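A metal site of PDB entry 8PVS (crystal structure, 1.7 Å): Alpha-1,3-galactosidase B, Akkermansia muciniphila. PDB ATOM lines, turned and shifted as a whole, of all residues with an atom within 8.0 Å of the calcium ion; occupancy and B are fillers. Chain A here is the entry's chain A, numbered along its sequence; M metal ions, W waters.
The backbone NH (N) of Arg 535 lies close to the side-chain carboxylate (OD2) of Asp 538, 2.9 Å away. N of Asn 499 is in hydrogen-bond range of O of Glu 504 (2.9 Å). The backbone NH of Gly 500 lies close to the side-chain carboxylate of Asp 538, 2.9 Å away. O of Ser 533 sits close to NH1 of Arg 535 (3.2 Å). The side-chain amide nitrogen of Asn 499 lies within hydrogen-bond range of the side-chain hydroxyl of Thr 502, at 3.0 Å.
Of the 16 residues printed, 3 come within 4 Å of the calcium ion.
The calcium ion is bound by the side-chain amide oxygen (OD1) of Asn 499 (2.4 Å), the backbone carbonyl oxygen (O) of Ser 533 (2.4 Å), water W1 (2.4 Å), the side-chain carboxylate (OD2) of Asp 538 (2.4 Å), water W3 (2.5 Å), water W2 (2.5 Å) and the side-chain carboxylate (OD1) of Asp 538 (2.8 Å).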
ATOM      1  N   PHE A 497      27.878 -32.377  -1.248  1.00  0.00           N
ATOM      2  CA  PHE A 497      27.848 -31.317  -2.259  1.00  0.00           C
ATOM      3  C   PHE A 497      26.569 -30.498  -2.144  1.00  0.00           C
ATOM      4  O   PHE A 497      25.532 -31.005  -1.714  1.00  0.00           O
ATOM      5  CB  PHE A 497      27.968 -31.915  -3.669  1.00  0.00           C
ATOM      6  CG  PHE A 497      29.214 -32.735  -3.853  1.00  0.00           C
ATOM      7  CD1 PHE A 497      30.451 -32.114  -3.942  1.00  0.00           C
ATOM      8  CD2 PHE A 497      29.155 -34.118  -3.904  1.00  0.00           C
ATOM      9  CE1 PHE A 497      31.609 -32.868  -4.094  1.00  0.00           C
ATOM     10  CE2 PHE A 497      30.302 -34.893  -4.052  1.00  0.00           C
ATOM     11  CZ  PHE A 497      31.539 -34.263  -4.153  1.00  0.00           C
ATOM     12  N   ILE A 498      26.667 -29.204  -2.485  1.00  0.00           N
ATOM     13  CA  ILE A 498      25.546 -28.277  -2.463  1.00  0.00           C
ATOM     14  C   ILE A 498      25.466 -27.604  -3.828  1.00  0.00           C
ATOM     15  O   ILE A 498      26.432 -26.967  -4.266  1.00  0.00           O
ATOM     16  CB  ILE A 498      25.676 -27.200  -1.375  1.00  0.00           C
ATOM     17  CG1 ILE A 498      25.976 -27.800  -0.008  1.00  0.00           C
ATOM     18  CG2 ILE A 498      24.415 -26.333  -1.340  1.00  0.00           C
ATOM     19  CD1 ILE A 498      26.553 -26.751   0.950  1.00  0.00           C
ATOM     20  N   ASN A 499      24.326 -27.714  -4.507  1.00  0.00           N
ATOM     21  CA  ASN A 499      24.179 -26.952  -5.742  1.00  0.00           C
ATOM     22  C   ASN A 499      24.057 -25.474  -5.396  1.00  0.00           C
ATOM     23  O   ASN A 499      23.137 -25.076  -4.671  1.00  0.00           O
ATOM     24  CB  ASN A 499      22.966 -27.407  -6.559  1.00  0.00           C
ATOM     25  CG  ASN A 499      22.916 -26.732  -7.904  1.00  0.00           C
ATOM     26  OD1 ASN A 499      23.854 -26.844  -8.683  1.00  0.00           O
ATOM     27  ND2 ASN A 499      21.847 -25.997  -8.158  1.00  0.00           N
ATOM     28  N   GLY A 500      25.013 -24.689  -5.857  1.00  0.00           N
ATOM     29  CA  GLY A 500      25.122 -23.293  -5.465  1.00  0.00           C
ATOM     30  C   GLY A 500      23.912 -22.423  -5.745  1.00  0.00           C
ATOM     31  O   GLY A 500      23.416 -21.734  -4.854  1.00  0.00           O
ATOM     32  N   PRO A 501      23.426 -22.432  -6.984  1.00  0.00           N
ATOM     33  CA  PRO A 501      22.334 -21.499  -7.327  1.00  0.00           C
ATOM     34  C   PRO A 501      21.057 -21.742  -6.546  1.00  0.00           C
ATOM     35  O   PRO A 501      20.280 -20.800  -6.373  1.00  0.00           O
ATOM     36  CB  PRO A 501      22.131 -21.749  -8.832  1.00  0.00           C
ATOM     37  CG  PRO A 501      23.448 -22.169  -9.322  1.00  0.00           C
ATOM     38  CD  PRO A 501      24.012 -23.028  -8.205  1.00  0.00           C
ATOM     39  N   THR A 502      20.802 -22.968  -6.089  1.00  0.00           N
ATOM     40  CA  THR A 502      19.509 -23.279  -5.488  1.00  0.00           C
ATOM     41  C   THR A 502      19.621 -23.737  -4.046  1.00  0.00           C
ATOM     42  O   THR A 502      18.608 -24.131  -3.471  1.00  0.00           O
ATOM     43  CB  THR A 502      18.757 -24.347  -6.296  1.00  0.00           C
ATOM     44  OG1 THR A 502      19.547 -25.544  -6.349  1.00  0.00           O
ATOM     45  CG2 THR A 502      18.475 -23.837  -7.722  1.00  0.00           C
ATOM     46  N   GLU A 504      20.804 -26.501  -2.708  1.00  0.00           N
ATOM     47  CA  GLU A 504      20.239 -27.846  -2.619  1.00  0.00           C
ATOM     48  C   GLU A 504      21.358 -28.833  -2.370  1.00  0.00           C
ATOM     49  O   GLU A 504      22.122 -29.153  -3.304  1.00  0.00           O
ATOM     50  CB  GLU A 504      19.472 -28.235  -3.884  1.00  0.00           C
ATOM     51  CG  GLU A 504      18.107 -27.575  -4.016  1.00  0.00           C
ATOM     52  CD  GLU A 504      17.458 -27.836  -5.374  1.00  0.00           C
ATOM     53  OE1 GLU A 504      18.018 -27.393  -6.409  1.00  0.00           O
ATOM     54  OE2 GLU A 504      16.398 -28.503  -5.394  1.00  0.00           O
ATOM     55  N   PRO A 531      30.165 -36.480  -8.907  1.00  0.00           N
ATOM     56  CA  PRO A 531      28.922 -36.362  -9.678  1.00  0.00           C
ATOM     57  C   PRO A 531      29.109 -35.311 -10.754  1.00  0.00           C
ATOM     58  O   PRO A 531      29.813 -34.316 -10.561  1.00  0.00           O
ATOM     59  CB  PRO A 531      27.891 -35.926  -8.632  1.00  0.00           C
ATOM     60  CG  PRO A 531      28.470 -36.369  -7.307  1.00  0.00           C
ATOM     61  CD  PRO A 531      29.966 -36.263  -7.467  1.00  0.00           C
ATOM     62  N   SER A 532      28.466 -35.522 -11.918  1.00  0.00           N
ATOM     63  CA  SER A 532      28.662 -34.585 -13.017  1.00  0.00           C
ATOM     64  C   SER A 532      28.028 -33.223 -12.751  1.00  0.00           C
ATOM     65  O   SER A 532      28.398 -32.248 -13.405  1.00  0.00           O
ATOM     66  CB  SER A 532      28.135 -35.172 -14.330  1.00  0.00           C
ATOM     67  OG  SER A 532      26.841 -35.708 -14.150  1.00  0.00           O
ATOM     68  N   SER A 533      27.105 -33.123 -11.788  1.00  0.00           N
ATOM     69  CA  SER A 533      26.483 -31.851 -11.448  1.00  0.00           C
ATOM     70  C   SER A 533      27.357 -30.945 -10.578  1.00  0.00           C
ATOM     71  O   SER A 533      27.001 -29.783 -10.371  1.00  0.00           O
ATOM     72  CB  SER A 533      25.153 -32.096 -10.745  1.00  0.00           C
ATOM     73  OG  SER A 533      25.360 -32.755  -9.497  1.00  0.00           O
ATOM     74  N   VAL A 534      28.492 -31.449 -10.079  1.00  0.00           N
ATOM     75  CA  VAL A 534      29.386 -30.650  -9.245  1.00  0.00           C
ATOM     76  C   VAL A 534      30.289 -29.797 -10.129  1.00  0.00           C
ATOM     77  O   VAL A 534      31.006 -30.328 -10.989  1.00  0.00           O
ATOM     78  CB  VAL A 534      30.205 -31.543  -8.302  1.00  0.00           C
ATOM     79  CG1 VAL A 534      31.216 -30.700  -7.518  1.00  0.00           C
ATOM     80  CG2 VAL A 534      29.273 -32.314  -7.349  1.00  0.00           C
ATOM     81  N   ARG A 535      30.253 -28.483  -9.933  1.00  0.00           N
ATOM     82  CA  ARG A 535      30.967 -27.548 -10.794  1.00  0.00           C
ATOM     83  C   ARG A 535      31.469 -26.369  -9.975  1.00  0.00           C
ATOM     84  O   ARG A 535      31.001 -26.120  -8.856  1.00  0.00           O
ATOM     85  CB  ARG A 535      30.073 -27.008 -11.933  1.00  0.00           C
ATOM     86  CG  ARG A 535      29.655 -28.054 -12.946  1.00  0.00           C
ATOM     87  CD  ARG A 535      28.655 -27.441 -13.931  1.00  0.00           C
ATOM     88  NE  ARG A 535      28.131 -28.441 -14.837  1.00  0.00           N
ATOM     89  CZ  ARG A 535      27.038 -29.170 -14.593  1.00  0.00           C
ATOM     90  NH1 ARG A 535      26.371 -29.030 -13.452  1.00  0.00           N
ATOM     91  NH2 ARG A 535      26.623 -30.038 -15.502  1.00  0.00           N
ATOM     92  N   ALA A 536      32.391 -25.614 -10.572  1.00  0.00           N
ATOM     93  CA  ALA A 536      32.735 -24.315 -10.020  1.00  0.00           C
ATOM     94  C   ALA A 536      31.450 -23.537  -9.778  1.00  0.00           C
ATOM     95  O   ALA A 536      30.556 -23.508 -10.617  1.00  0.00           O
ATOM     96  CB  ALA A 536      33.657 -23.542 -10.964  1.00  0.00           C
ATOM     97  N   GLY A 537      31.353 -22.934  -8.602  1.00  0.00           N
ATOM     98  CA  GLY A 537      30.154 -22.251  -8.186  1.00  0.00           C
ATOM     99  C   GLY A 537      29.272 -23.043  -7.241  1.00  0.00           C
ATOM    100  O   GLY A 537      28.389 -22.466  -6.605  1.00  0.00           O
ATOM    101  N   ASP A 538      29.497 -24.341  -7.141  1.00  0.00           N
ATOM    102  CA  ASP A 538      28.838 -25.097  -6.096  1.00  0.00           C
ATOM    103  C   ASP A 538      29.596 -24.903  -4.781  1.00  0.00           C
ATOM    104  O   ASP A 538      30.578 -24.155  -4.691  1.00  0.00           O
ATOM    105  CB  ASP A 538      28.728 -26.566  -6.507  1.00  0.00           C
ATOM    106  CG  ASP A 538      27.715 -26.794  -7.638  1.00  0.00           C
ATOM    107  OD1 ASP A 538      26.809 -25.956  -7.810  1.00  0.00           O
ATOM    108  OD2 ASP A 538      27.856 -27.786  -8.381  1.00  0.00           O
ATOM    109  N   ALA A 539      29.127 -25.565  -3.726  1.00  0.00           N
ATOM    110  CA  ALA A 539      29.755 -25.483  -2.411  1.00  0.00           C
ATOM    111  C   ALA A 539      29.834 -26.892  -1.835  1.00  0.00           C
ATOM    112  O   ALA A 539      29.161 -27.806  -2.304  1.00  0.00           O
ATOM    113  CB  ALA A 539      28.991 -24.553  -1.458  1.00  0.00           C
HETATM  114 CA    CA M   1      25.753 -27.977  -9.486  1.00  0.00          CA
HETATM  115  O   HOH W   1      25.273 -29.598  -7.820  1.00  0.00           O
HETATM  116  O   HOH W   2      24.159 -28.533 -11.360  1.00  0.00           O
HETATM  117  O   HOH W   3      26.380 -26.349 -11.249  1.00  0.00           O
